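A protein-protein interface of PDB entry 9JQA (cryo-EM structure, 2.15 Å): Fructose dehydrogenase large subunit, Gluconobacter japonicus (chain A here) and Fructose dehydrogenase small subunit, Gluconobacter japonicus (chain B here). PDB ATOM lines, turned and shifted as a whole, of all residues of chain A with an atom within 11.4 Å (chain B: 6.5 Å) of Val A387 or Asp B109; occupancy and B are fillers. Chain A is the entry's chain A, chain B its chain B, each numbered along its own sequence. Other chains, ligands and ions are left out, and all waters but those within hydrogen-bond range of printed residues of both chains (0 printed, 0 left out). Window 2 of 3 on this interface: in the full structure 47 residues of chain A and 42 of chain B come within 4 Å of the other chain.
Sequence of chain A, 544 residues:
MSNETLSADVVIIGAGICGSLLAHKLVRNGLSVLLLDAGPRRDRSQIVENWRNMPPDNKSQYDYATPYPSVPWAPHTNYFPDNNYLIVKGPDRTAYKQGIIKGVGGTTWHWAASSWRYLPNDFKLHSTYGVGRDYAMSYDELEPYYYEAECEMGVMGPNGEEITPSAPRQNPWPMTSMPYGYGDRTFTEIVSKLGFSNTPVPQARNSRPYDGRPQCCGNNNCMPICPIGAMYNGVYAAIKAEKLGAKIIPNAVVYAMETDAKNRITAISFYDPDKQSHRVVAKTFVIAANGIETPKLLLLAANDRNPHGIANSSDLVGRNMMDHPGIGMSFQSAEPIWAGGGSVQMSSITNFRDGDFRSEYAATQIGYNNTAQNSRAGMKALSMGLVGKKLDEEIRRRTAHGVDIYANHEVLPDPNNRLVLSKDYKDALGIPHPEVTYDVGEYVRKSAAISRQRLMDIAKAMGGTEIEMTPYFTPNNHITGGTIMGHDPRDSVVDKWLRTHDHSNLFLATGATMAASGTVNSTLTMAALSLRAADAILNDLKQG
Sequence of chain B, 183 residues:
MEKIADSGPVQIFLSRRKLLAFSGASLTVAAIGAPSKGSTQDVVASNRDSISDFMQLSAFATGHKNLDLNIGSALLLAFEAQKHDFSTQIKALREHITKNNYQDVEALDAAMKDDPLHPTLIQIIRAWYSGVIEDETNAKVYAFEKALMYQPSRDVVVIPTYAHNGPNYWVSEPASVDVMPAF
The side-chain carboxylate (OE2) of Glu B106 sits at hydrogen-bond distance from the backbone NH (N) of Lys A389. The side-chain hydroxyl of Tyr B129 is in hydrogen-bond range of the side-chain carboxylate of Asp A392, 2.7 Å away.
The backbone carbonyl oxygen (O) of Thr B62 sits at hydrogen-bond distance from the side-chain hydroxyl (OH) of Tyr B129, at 3.5 Å. NE2 of His B118 lies within hydrogen-bond range of OD1 of Asp B109, at 2.6 Å.
CB of Tyr B129 touches CD2 of Leu A382, at 3.8 Å. Val B105 touches Val A387 (O to CG2, 3.8 Å). Glu B106 touches Val A387. CG2 of Val A387 touches CB of Asp B109, 3.7 Å away. Ile B122 touches Val A387. Ile B125 touches Val A387. Val B105 touches Gly A388 (CG1 to N, 3.6 Å). CG2 of Ile B125 touches CD2 of Leu A391 (3.8 Å). Leu A391 touches Tyr B129 (CD2 to CZ, 3.7 Å). Tyr B129 touches Ile A395.
Of the printed residues of chain B, Val A387 touches Val B105, Glu B106, Asp B109, Ile B122 and Ile B125. Asp B109 touches just one residue of chain A: Val A387 (3.7 Å). Of the printed residues of chain A, Val B105 touches Val A387 (3.8 Å) and Gly A388 (3.6 Å). Of the printed residues of chain A, Glu B106 touches Val A387 (3.8 Å), Gly A388 (3.2 Å) and Lys A389 (2.8 Å). Ala B107 touches none of the printed residues of chain A. Leu B108 touches none of the printed residues of chain A. Ala B110 touches none of the printed residues of chain A. No residue of chain A comes within 4 Å of Met B112. No residue of chain A comes within 4 Å of Lys B113. Of the printed residues of chain A, Ile B122 touches Val A387. Of the printed residues of chain B, Ile A395 touches Tyr B129. Of the printed residues of chain A, Tyr B129 touches Leu A382 (3.8 Å), Leu A391 (3.7 Å), Asp A392 (2.7 Å) and Ile A395 (3.8 Å). Of the printed residues of chain B, Leu A382 touches Tyr B129. Of the printed residues of chain B, Asp A392 touches Tyr B129 (2.7 Å). Of the printed residues of chain B, Leu A391 touches Ile B125 and Tyr B129. Glu A394 touches none of the printed residues of chain B. Ala A377 touches none of the printed residues of chain B. The nearest printed residue of chain B that does not touch Leu A391 is Glu B106 (6.2 Å).
Printed residues of chain B that touch a printed residue of chain A: Val B105, Glu B106, Asp B109, Ile B122, Ile B125 and Tyr B129. Of the 19 printed residues of chain A, 7 touch a printed residue of chain B. Printed residues of chain A that touch a printed residue of chain B: Leu A382, Val A387, Gly A388, Lys A389, Leu A391, Asp A392 and Ile A395. Hydrophobic or aromatic side chains of chain A within 4 Å of the printed part of chain B: Leu A382, Val A387, Leu A391 and Ile A395. Among the printed residues, 13 pairs touch across the chains.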
ATOM      1  N   ALA A 377     -24.029  -3.518  15.946  1.00  0.00           N
ATOM      2  CA  ALA A 377     -22.615  -3.170  15.894  1.00  0.00           C
ATOM      3  C   ALA A 377     -21.758  -4.386  15.587  1.00  0.00           C
ATOM      4  O   ALA A 377     -20.828  -4.310  14.778  1.00  0.00           O
ATOM      5  CB  ALA A 377     -22.182  -2.540  17.214  1.00  0.00           C
ATOM      6  N   GLY A 378     -22.053  -5.517  16.228  1.00  0.00           N
ATOM      7  CA  GLY A 378     -21.270  -6.714  15.989  1.00  0.00           C
ATOM      8  C   GLY A 378     -21.377  -7.196  14.558  1.00  0.00           C
ATOM      9  O   GLY A 378     -20.371  -7.509  13.920  1.00  0.00           O
ATOM     10  N   MET A 379     -22.600  -7.245  14.028  1.00  0.00           N
ATOM     11  CA  MET A 379     -22.778  -7.693  12.652  1.00  0.00           C
ATOM     12  C   MET A 379     -22.113  -6.738  11.669  1.00  0.00           C
ATOM     13  O   MET A 379     -21.468  -7.177  10.710  1.00  0.00           O
ATOM     14  CB  MET A 379     -24.263  -7.851  12.337  1.00  0.00           C
ATOM     15  CG  MET A 379     -24.950  -8.930  13.155  1.00  0.00           C
ATOM     16  SD  MET A 379     -24.020 -10.471  13.227  1.00  0.00           S
ATOM     17  CE  MET A 379     -24.128 -11.019  11.529  1.00  0.00           C
ATOM     18  N   LYS A 380     -22.244  -5.429  11.893  1.00  0.00           N
ATOM     19  CA  LYS A 380     -21.625  -4.466  10.989  1.00  0.00           C
ATOM     20  C   LYS A 380     -20.106  -4.567  11.023  1.00  0.00           C
ATOM     21  O   LYS A 380     -19.452  -4.569   9.972  1.00  0.00           O
ATOM     22  CB  LYS A 380     -22.079  -3.053  11.344  1.00  0.00           C
ATOM     23  CG  LYS A 380     -21.369  -1.965  10.570  1.00  0.00           C
ATOM     24  CD  LYS A 380     -21.827  -1.925   9.128  1.00  0.00           C
ATOM     25  CE  LYS A 380     -21.272  -0.709   8.417  1.00  0.00           C
ATOM     26  NZ  LYS A 380     -20.394  -1.086   7.281  1.00  0.00           N
ATOM     27  N   ALA A 381     -19.523  -4.663  12.219  1.00  0.00           N
ATOM     28  CA  ALA A 381     -18.073  -4.767  12.327  1.00  0.00           C
ATOM     29  C   ALA A 381     -17.565  -6.070  11.726  1.00  0.00           C
ATOM     30  O   ALA A 381     -16.494  -6.097  11.111  1.00  0.00           O
ATOM     31  CB  ALA A 381     -17.645  -4.643  13.786  1.00  0.00           C
ATOM     32  N   LEU A 382     -18.309  -7.164  11.901  1.00  0.00           N
ATOM     33  CA  LEU A 382     -17.915  -8.423  11.281  1.00  0.00           C
ATOM     34  C   LEU A 382     -17.976  -8.331   9.763  1.00  0.00           C
ATOM     35  O   LEU A 382     -17.094  -8.850   9.070  1.00  0.00           O
ATOM     36  CB  LEU A 382     -18.801  -9.556  11.791  1.00  0.00           C
ATOM     37  CG  LEU A 382     -18.477 -10.048  13.200  1.00  0.00           C
ATOM     38  CD1 LEU A 382     -19.556 -10.992  13.691  1.00  0.00           C
ATOM     39  CD2 LEU A 382     -17.114 -10.713  13.232  1.00  0.00           C
ATOM     40  N   SER A 383     -19.006  -7.675   9.228  1.00  0.00           N
ATOM     41  CA  SER A 383     -19.093  -7.478   7.788  1.00  0.00           C
ATOM     42  C   SER A 383     -18.021  -6.529   7.271  1.00  0.00           C
ATOM     43  O   SER A 383     -17.709  -6.558   6.077  1.00  0.00           O
ATOM     44  CB  SER A 383     -20.475  -6.952   7.410  1.00  0.00           C
ATOM     45  OG  SER A 383     -20.526  -5.540   7.515  1.00  0.00           O
ATOM     46  N   MET A 384     -17.458  -5.687   8.137  1.00  0.00           N
ATOM     47  CA  MET A 384     -16.394  -4.784   7.717  1.00  0.00           C
ATOM     48  C   MET A 384     -15.069  -5.497   7.484  1.00  0.00           C
ATOM     49  O   MET A 384     -14.145  -4.882   6.942  1.00  0.00           O
ATOM     50  CB  MET A 384     -16.207  -3.680   8.754  1.00  0.00           C
ATOM     51  CG  MET A 384     -17.083  -2.468   8.523  1.00  0.00           C
ATOM     52  SD  MET A 384     -17.066  -1.331   9.916  1.00  0.00           S
ATOM     53  CE  MET A 384     -15.482  -0.538   9.672  1.00  0.00           C
ATOM     54  N   GLY A 385     -14.948  -6.762   7.877  1.00  0.00           N
ATOM     55  CA  GLY A 385     -13.720  -7.499   7.657  1.00  0.00           C
ATOM     56  C   GLY A 385     -12.587  -7.167   8.600  1.00  0.00           C
ATOM     57  O   GLY A 385     -11.420  -7.261   8.210  1.00  0.00           O
ATOM     58  N   LEU A 386     -12.893  -6.783   9.833  1.00  0.00           N
ATOM     59  CA  LEU A 386     -11.883  -6.426  10.817  1.00  0.00           C
ATOM     60  C   LEU A 386     -11.583  -7.609  11.726  1.00  0.00           C
ATOM     61  O   LEU A 386     -12.446  -8.450  11.989  1.00  0.00           O
ATOM     62  CB  LEU A 386     -12.337  -5.231  11.652  1.00  0.00           C
ATOM     63  CG  LEU A 386     -12.703  -3.979  10.860  1.00  0.00           C
ATOM     64  CD1 LEU A 386     -13.567  -3.070  11.696  1.00  0.00           C
ATOM     65  CD2 LEU A 386     -11.454  -3.256  10.405  1.00  0.00           C
ATOM     66  N   VAL A 387     -10.339  -7.673  12.200  1.00  0.00           N
ATOM     67  CA  VAL A 387      -9.880  -8.752  13.064  1.00  0.00           C
ATOM     68  C   VAL A 387      -9.124  -8.159  14.244  1.00  0.00           C
ATOM     69  O   VAL A 387      -8.652  -7.022  14.205  1.00  0.00           O
ATOM     70  CB  VAL A 387      -8.985  -9.764  12.315  1.00  0.00           C
ATOM     71  CG1 VAL A 387      -9.705 -10.322  11.104  1.00  0.00           C
ATOM     72  CG2 VAL A 387      -7.678  -9.115  11.907  1.00  0.00           C
ATOM     73  N   GLY A 388      -9.018  -8.954  15.305  1.00  0.00           N
ATOM     74  CA  GLY A 388      -8.172  -8.581  16.426  1.00  0.00           C
ATOM     75  C   GLY A 388      -8.739  -7.428  17.229  1.00  0.00           C
ATOM     76  O   GLY A 388      -9.951  -7.307  17.427  1.00  0.00           O
ATOM     77  N   LYS A 389      -7.838  -6.571  17.713  1.00  0.00           N
ATOM     78  CA  LYS A 389      -8.254  -5.443  18.538  1.00  0.00           C
ATOM     79  C   LYS A 389      -9.080  -4.440  17.749  1.00  0.00           C
ATOM     80  O   LYS A 389      -9.940  -3.765  18.322  1.00  0.00           O
ATOM     81  CB  LYS A 389      -7.031  -4.760  19.147  1.00  0.00           C
ATOM     82  CG  LYS A 389      -6.518  -5.428  20.405  1.00  0.00           C
ATOM     83  CD  LYS A 389      -5.014  -5.619  20.353  1.00  0.00           C
ATOM     84  CE  LYS A 389      -4.423  -5.693  21.748  1.00  0.00           C
ATOM     85  NZ  LYS A 389      -5.373  -6.307  22.714  1.00  0.00           N
ATOM     86  N   LYS A 390      -8.828  -4.319  16.444  1.00  0.00           N
ATOM     87  CA  LYS A 390      -9.618  -3.408  15.624  1.00  0.00           C
ATOM     88  C   LYS A 390     -11.080  -3.829  15.589  1.00  0.00           C
ATOM     89  O   LYS A 390     -11.977  -2.981  15.642  1.00  0.00           O
ATOM     90  CB  LYS A 390      -9.045  -3.341  14.212  1.00  0.00           C
ATOM     91  CG  LYS A 390      -7.563  -3.032  14.163  1.00  0.00           C
ATOM     92  CD  LYS A 390      -7.311  -1.606  13.707  1.00  0.00           C
ATOM     93  CE  LYS A 390      -7.306  -0.645  14.881  1.00  0.00           C
ATOM     94  NZ  LYS A 390      -6.719   0.673  14.520  1.00  0.00           N
ATOM     95  N   LEU A 391     -11.340  -5.134  15.497  1.00  0.00           N
ATOM     96  CA  LEU A 391     -12.716  -5.617  15.499  1.00  0.00           C
ATOM     97  C   LEU A 391     -13.416  -5.296  16.813  1.00  0.00           C
ATOM     98  O   LEU A 391     -14.566  -4.841  16.818  1.00  0.00           O
ATOM     99  CB  LEU A 391     -12.737  -7.121  15.235  1.00  0.00           C
ATOM    100  CG  LEU A 391     -14.092  -7.824  15.275  1.00  0.00           C
ATOM    101  CD1 LEU A 391     -15.022  -7.255  14.226  1.00  0.00           C
ATOM    102  CD2 LEU A 391     -13.911  -9.312  15.077  1.00  0.00           C
ATOM    103  N   ASP A 392     -12.739  -5.526  17.939  1.00  0.00           N
ATOM    104  CA  ASP A 392     -13.333  -5.222  19.237  1.00  0.00           C
ATOM    105  C   ASP A 392     -13.593  -3.730  19.391  1.00  0.00           C
ATOM    106  O   ASP A 392     -14.654  -3.322  19.881  1.00  0.00           O
ATOM    107  CB  ASP A 392     -12.423  -5.720  20.358  1.00  0.00           C
ATOM    108  CG  ASP A 392     -12.358  -7.226  20.429  1.00  0.00           C
ATOM    109  OD1 ASP A 392     -13.349  -7.884  20.056  1.00  0.00           O
ATOM    110  OD2 ASP A 392     -11.315  -7.755  20.859  1.00  0.00           O
ATOM    111  N   GLU A 393     -12.631  -2.902  18.979  1.00  0.00           N
ATOM    112  CA  GLU A 393     -12.808  -1.458  19.067  1.00  0.00           C
ATOM    113  C   GLU A 393     -13.966  -0.995  18.198  1.00  0.00           C
ATOM    114  O   GLU A 393     -14.748  -0.132  18.607  1.00  0.00           O
ATOM    115  CB  GLU A 393     -11.521  -0.743  18.665  1.00  0.00           C
ATOM    116  CG  GLU A 393     -10.416  -0.838  19.693  1.00  0.00           C
ATOM    117  CD  GLU A 393      -9.048  -0.609  19.092  1.00  0.00           C
ATOM    118  OE1 GLU A 393      -8.975  -0.207  17.912  1.00  0.00           O
ATOM    119  OE2 GLU A 393      -8.043  -0.833  19.797  1.00  0.00           O
ATOM    120  N   GLU A 394     -14.090  -1.553  16.992  1.00  0.00           N
ATOM    121  CA  GLU A 394     -15.196  -1.182  16.121  1.00  0.00           C
ATOM    122  C   GLU A 394     -16.533  -1.594  16.717  1.00  0.00           C
ATOM    123  O   GLU A 394     -17.502  -0.832  16.663  1.00  0.00           O
ATOM    124  CB  GLU A 394     -15.013  -1.808  14.742  1.00  0.00           C
ATOM    125  CG  GLU A 394     -16.015  -1.319  13.720  1.00  0.00           C
ATOM    126  CD  GLU A 394     -15.688   0.063  13.207  1.00  0.00           C
ATOM    127  OE1 GLU A 394     -14.546   0.521  13.409  1.00  0.00           O
ATOM    128  OE2 GLU A 394     -16.574   0.697  12.602  1.00  0.00           O
ATOM    129  N   ILE A 395     -16.606  -2.799  17.286  1.00  0.00           N
ATOM    130  CA  ILE A 395     -17.853  -3.244  17.903  1.00  0.00           C
ATOM    131  C   ILE A 395     -18.238  -2.311  19.042  1.00  0.00           C
ATOM    132  O   ILE A 395     -19.387  -1.864  19.141  1.00  0.00           O
ATOM    133  CB  ILE A 395     -17.728  -4.698  18.387  1.00  0.00           C
ATOM    134  CG1 ILE A 395     -17.669  -5.657  17.202  1.00  0.00           C
ATOM    135  CG2 ILE A 395     -18.897  -5.056  19.278  1.00  0.00           C
ATOM    136  CD1 ILE A 395     -17.094  -7.005  17.543  1.00  0.00           C
ATOM    137  N   ALA B  61      -7.145 -16.600  16.449  1.00  0.00           N
ATOM    138  CA  ALA B  61      -7.856 -15.787  15.470  1.00  0.00           C
ATOM    139  C   ALA B  61      -8.721 -14.729  16.138  1.00  0.00           C
ATOM    140  O   ALA B  61      -8.749 -13.575  15.698  1.00  0.00           O
ATOM    141  CB  ALA B  61      -8.708 -16.680  14.571  1.00  0.00           C
ATOM    142  N   THR B  62      -9.444 -15.101  17.188  1.00  0.00           N
ATOM    143  CA  THR B  62     -10.248 -14.126  17.908  1.00  0.00           C
ATOM    144  C   THR B  62      -9.404 -13.219  18.787  1.00  0.00           C
ATOM    145  O   THR B  62      -9.872 -12.145  19.178  1.00  0.00           O
ATOM    146  CB  THR B  62     -11.296 -14.834  18.764  1.00  0.00           C
ATOM    147  OG1 THR B  62     -10.644 -15.596  19.786  1.00  0.00           O
ATOM    148  CG2 THR B  62     -12.135 -15.764  17.912  1.00  0.00           C
ATOM    149  N   TYR B 102       3.674 -15.752  13.125  1.00  0.00           N
ATOM    150  CA  TYR B 102       2.773 -14.623  13.309  1.00  0.00           C
ATOM    151  C   TYR B 102       2.430 -14.469  14.782  1.00  0.00           C
ATOM    152  O   TYR B 102       2.119 -15.447  15.466  1.00  0.00           O
ATOM    153  CB  TYR B 102       1.502 -14.818  12.484  1.00  0.00           C
ATOM    154  CG  TYR B 102       1.736 -14.864  10.994  1.00  0.00           C
ATOM    155  CD1 TYR B 102       2.468 -13.876  10.356  1.00  0.00           C
ATOM    156  CD2 TYR B 102       1.220 -15.895  10.225  1.00  0.00           C
ATOM    157  CE1 TYR B 102       2.682 -13.915   8.995  1.00  0.00           C
ATOM    158  CE2 TYR B 102       1.429 -15.941   8.864  1.00  0.00           C
ATOM    159  CZ  TYR B 102       2.159 -14.950   8.254  1.00  0.00           C
ATOM    160  OH  TYR B 102       2.369 -14.996   6.897  1.00  0.00           O
ATOM    161  N   ASP B 104      -0.014 -12.306  16.120  1.00  0.00           N
ATOM    162  CA  ASP B 104      -1.429 -12.097  16.382  1.00  0.00           C
ATOM    163  C   ASP B 104      -2.201 -12.283  15.086  1.00  0.00           C
ATOM    164  O   ASP B 104      -1.622 -12.447  14.010  1.00  0.00           O
ATOM    165  CB  ASP B 104      -1.691 -10.712  16.981  1.00  0.00           C
ATOM    166  CG  ASP B 104      -0.955  -9.610  16.249  1.00  0.00           C
ATOM    167  OD1 ASP B 104      -0.507  -9.853  15.111  1.00  0.00           O
ATOM    168  OD2 ASP B 104      -0.823  -8.500  16.806  1.00  0.00           O
ATOM    169  N   VAL B 105      -3.530 -12.258  15.204  1.00  0.00           N
ATOM    170  CA  VAL B 105      -4.379 -12.420  14.033  1.00  0.00           C
ATOM    171  C   VAL B 105      -4.250 -11.241  13.079  1.00  0.00           C
ATOM    172  O   VAL B 105      -4.563 -11.375  11.894  1.00  0.00           O
ATOM    173  CB  VAL B 105      -5.844 -12.629  14.460  1.00  0.00           C
ATOM    174  CG1 VAL B 105      -6.411 -11.359  15.049  1.00  0.00           C
ATOM    175  CG2 VAL B 105      -6.684 -13.096  13.287  1.00  0.00           C
ATOM    176  N   GLU B 106      -3.787 -10.086  13.559  1.00  0.00           N
ATOM    177  CA  GLU B 106      -3.620  -8.936  12.676  1.00  0.00           C
ATOM    178  C   GLU B 106      -2.574  -9.217  11.604  1.00  0.00           C
ATOM    179  O   GLU B 106      -2.818  -9.004  10.411  1.00  0.00           O
ATOM    180  CB  GLU B 106      -3.240  -7.703  13.493  1.00  0.00           C
ATOM    181  CG  GLU B 106      -4.422  -6.990  14.122  1.00  0.00           C
ATOM    182  CD  GLU B 106      -4.772  -7.532  15.493  1.00  0.00           C
ATOM    183  OE1 GLU B 106      -4.365  -8.667  15.811  1.00  0.00           O
ATOM    184  OE2 GLU B 106      -5.453  -6.819  16.257  1.00  0.00           O
ATOM    185  N   ALA B 107      -1.403  -9.707  12.013  1.00  0.00           N
ATOM    186  CA  ALA B 107      -0.351 -10.016  11.050  1.00  0.00           C
ATOM    187  C   ALA B 107      -0.770 -11.144  10.118  1.00  0.00           C
ATOM    188  O   ALA B 107      -0.500 -11.095   8.912  1.00  0.00           O
ATOM    189  CB  ALA B 107       0.940 -10.378  11.782  1.00  0.00           C
ATOM    190  N   LEU B 108      -1.423 -12.172  10.662  1.00  0.00           N
ATOM    191  CA  LEU B 108      -1.868 -13.285   9.833  1.00  0.00           C
ATOM    192  C   LEU B 108      -2.881 -12.828   8.794  1.00  0.00           C
ATOM    193  O   LEU B 108      -2.800 -13.217   7.626  1.00  0.00           O
ATOM    194  CB  LEU B 108      -2.458 -14.386  10.713  1.00  0.00           C
ATOM    195  CG  LEU B 108      -3.197 -15.514   9.997  1.00  0.00           C
ATOM    196  CD1 LEU B 108      -2.215 -16.467   9.343  1.00  0.00           C
ATOM    197  CD2 LEU B 108      -4.094 -16.255  10.969  1.00  0.00           C
ATOM    198  N   ASP B 109      -3.834 -11.989   9.199  1.00  0.00           N
ATOM    199  CA  ASP B 109      -4.831 -11.484   8.264  1.00  0.00           C
ATOM    200  C   ASP B 109      -4.198 -10.570   7.222  1.00  0.00           C
ATOM    201  O   ASP B 109      -4.608 -10.574   6.057  1.00  0.00           O
ATOM    202  CB  ASP B 109      -5.935 -10.755   9.026  1.00  0.00           C
ATOM    203  CG  ASP B 109      -6.863  -9.984   8.114  1.00  0.00           C
ATOM    204  OD1 ASP B 109      -7.579 -10.622   7.316  1.00  0.00           O
ATOM    205  OD2 ASP B 109      -6.879  -8.739   8.197  1.00  0.00           O
ATOM    206  N   ALA B 110      -3.205  -9.774   7.625  1.00  0.00           N
ATOM    207  CA  ALA B 110      -2.517  -8.918   6.665  1.00  0.00           C
ATOM    208  C   ALA B 110      -1.764  -9.741   5.628  1.00  0.00           C
ATOM    209  O   ALA B 110      -1.789  -9.422   4.434  1.00  0.00           O
ATOM    210  CB  ALA B 110      -1.563  -7.973   7.396  1.00  0.00           C
ATOM    211  N   ALA B 111      -1.090 -10.806   6.063  1.00  0.00           N
ATOM    212  CA  ALA B 111      -0.312 -11.623   5.141  1.00  0.00           C
ATOM    213  C   ALA B 111      -1.162 -12.624   4.370  1.00  0.00           C
ATOM    214  O   ALA B 111      -0.688 -13.181   3.375  1.00  0.00           O
ATOM    215  CB  ALA B 111       0.788 -12.365   5.900  1.00  0.00           C
ATOM    216  N   MET B 112      -2.398 -12.862   4.802  1.00  0.00           N
ATOM    217  CA  MET B 112      -3.279 -13.842   4.186  1.00  0.00           C
ATOM    218  C   MET B 112      -4.309 -13.198   3.262  1.00  0.00           C
ATOM    219  O   MET B 112      -5.332 -13.815   2.958  1.00  0.00           O
ATOM    220  CB  MET B 112      -3.965 -14.659   5.286  1.00  0.00           C
ATOM    221  CG  MET B 112      -4.625 -15.954   4.845  1.00  0.00           C
ATOM    222  SD  MET B 112      -4.277 -17.340   5.931  1.00  0.00           S
ATOM    223  CE  MET B 112      -2.511 -17.496   5.702  1.00  0.00           C
ATOM    224  N   LYS B 113      -4.053 -11.977   2.792  1.00  0.00           N
ATOM    225  CA  LYS B 113      -5.081 -11.245   2.056  1.00  0.00           C
ATOM    226  C   LYS B 113      -5.511 -11.987   0.796  1.00  0.00           C
ATOM    227  O   LYS B 113      -6.706 -12.059   0.488  1.00  0.00           O
ATOM    228  CB  LYS B 113      -4.582  -9.842   1.713  1.00  0.00           C
ATOM    229  CG  LYS B 113      -4.873  -8.809   2.789  1.00  0.00           C
ATOM    230  CD  LYS B 113      -6.331  -8.862   3.222  1.00  0.00           C
ATOM    231  CE  LYS B 113      -6.564  -8.055   4.487  1.00  0.00           C
ATOM    232  NZ  LYS B 113      -7.904  -7.408   4.495  1.00  0.00           N
ATOM    233  N   ASP B 114      -4.557 -12.545   0.053  1.00  0.00           N
ATOM    234  CA  ASP B 114      -4.858 -13.257  -1.182  1.00  0.00           C
ATOM    235  C   ASP B 114      -4.844 -14.772  -1.024  1.00  0.00           C
ATOM    236  O   ASP B 114      -5.094 -15.482  -2.003  1.00  0.00           O
ATOM    237  CB  ASP B 114      -3.873 -12.844  -2.279  1.00  0.00           C
ATOM    238  CG  ASP B 114      -3.768 -11.341  -2.433  1.00  0.00           C
ATOM    239  OD1 ASP B 114      -4.069 -10.620  -1.459  1.00  0.00           O
ATOM    240  OD2 ASP B 114      -3.387 -10.877  -3.529  1.00  0.00           O
ATOM    241  N   HIS B 118      -7.751 -17.583   3.778  1.00  0.00           N
ATOM    242  CA  HIS B 118      -8.291 -16.412   4.463  1.00  0.00           C
ATOM    243  C   HIS B 118      -9.797 -16.482   4.702  1.00  0.00           C
ATOM    244  O   HIS B 118     -10.236 -16.104   5.806  1.00  0.00           O
ATOM    245  CB  HIS B 118      -7.914 -15.164   3.657  1.00  0.00           C
ATOM    246  CG  HIS B 118      -8.368 -13.877   4.266  1.00  0.00           C
ATOM    247  ND1 HIS B 118      -9.458 -13.176   3.799  1.00  0.00           N
ATOM    248  CD2 HIS B 118      -7.861 -13.148   5.289  1.00  0.00           C
ATOM    249  CE1 HIS B 118      -9.610 -12.077   4.515  1.00  0.00           C
ATOM    250  NE2 HIS B 118      -8.654 -12.037   5.426  1.00  0.00           N
ATOM    251  N   LEU B 121     -10.458 -18.390   7.882  1.00  0.00           N
ATOM    252  CA  LEU B 121     -10.104 -17.616   9.068  1.00  0.00           C
ATOM    253  C   LEU B 121     -11.198 -16.616   9.414  1.00  0.00           C
ATOM    254  O   LEU B 121     -11.613 -16.507  10.579  1.00  0.00           O
ATOM    255  CB  LEU B 121      -8.777 -16.893   8.843  1.00  0.00           C
ATOM    256  CG  LEU B 121      -8.354 -15.927   9.946  1.00  0.00           C
ATOM    257  CD1 LEU B 121      -7.734 -16.686  11.098  1.00  0.00           C
ATOM    258  CD2 LEU B 121      -7.397 -14.870   9.419  1.00  0.00           C
ATOM    259  N   ILE B 122     -11.690 -15.890   8.411  1.00  0.00           N
ATOM    260  CA  ILE B 122     -12.736 -14.907   8.668  1.00  0.00           C
ATOM    261  C   ILE B 122     -14.019 -15.597   9.116  1.00  0.00           C
ATOM    262  O   ILE B 122     -14.741 -15.089   9.979  1.00  0.00           O
ATOM    263  CB  ILE B 122     -12.955 -14.027   7.426  1.00  0.00           C
ATOM    264  CG1 ILE B 122     -11.661 -13.298   7.074  1.00  0.00           C
ATOM    265  CG2 ILE B 122     -14.060 -13.024   7.671  1.00  0.00           C
ATOM    266  CD1 ILE B 122     -11.096 -12.478   8.213  1.00  0.00           C
ATOM    267  N   ILE B 125     -13.659 -16.522  12.793  1.00  0.00           N
ATOM    268  CA  ILE B 125     -13.833 -15.336  13.628  1.00  0.00           C
ATOM    269  C   ILE B 125     -15.305 -14.950  13.703  1.00  0.00           C
ATOM    270  O   ILE B 125     -15.819 -14.614  14.777  1.00  0.00           O
ATOM    271  CB  ILE B 125     -12.968 -14.177  13.103  1.00  0.00           C
ATOM    272  CG1 ILE B 125     -11.487 -14.508  13.264  1.00  0.00           C
ATOM    273  CG2 ILE B 125     -13.299 -12.896  13.835  1.00  0.00           C
ATOM    274  CD1 ILE B 125     -10.589 -13.707  12.365  1.00  0.00           C
ATOM    275  N   TYR B 129     -17.658 -14.776  17.035  1.00  0.00           N
ATOM    276  CA  TYR B 129     -18.140 -13.470  17.465  1.00  0.00           C
ATOM    277  C   TYR B 129     -19.658 -13.367  17.394  1.00  0.00           C
ATOM    278  O   TYR B 129     -20.286 -12.858  18.325  1.00  0.00           O
ATOM    279  CB  TYR B 129     -17.487 -12.369  16.631  1.00  0.00           C
ATOM    280  CG  TYR B 129     -16.244 -11.806  17.271  1.00  0.00           C
ATOM    281  CD1 TYR B 129     -15.020 -12.434  17.118  1.00  0.00           C
ATOM    282  CD2 TYR B 129     -16.297 -10.659  18.044  1.00  0.00           C
ATOM    283  CE1 TYR B 129     -13.884 -11.932  17.708  1.00  0.00           C
ATOM    284  CE2 TYR B 129     -15.166 -10.149  18.640  1.00  0.00           C
ATOM    285  CZ  TYR B 129     -13.961 -10.790  18.467  1.00  0.00           C
ATOM    286  OH  TYR B 129     -12.829 -10.286  19.056  1.00  0.00           O
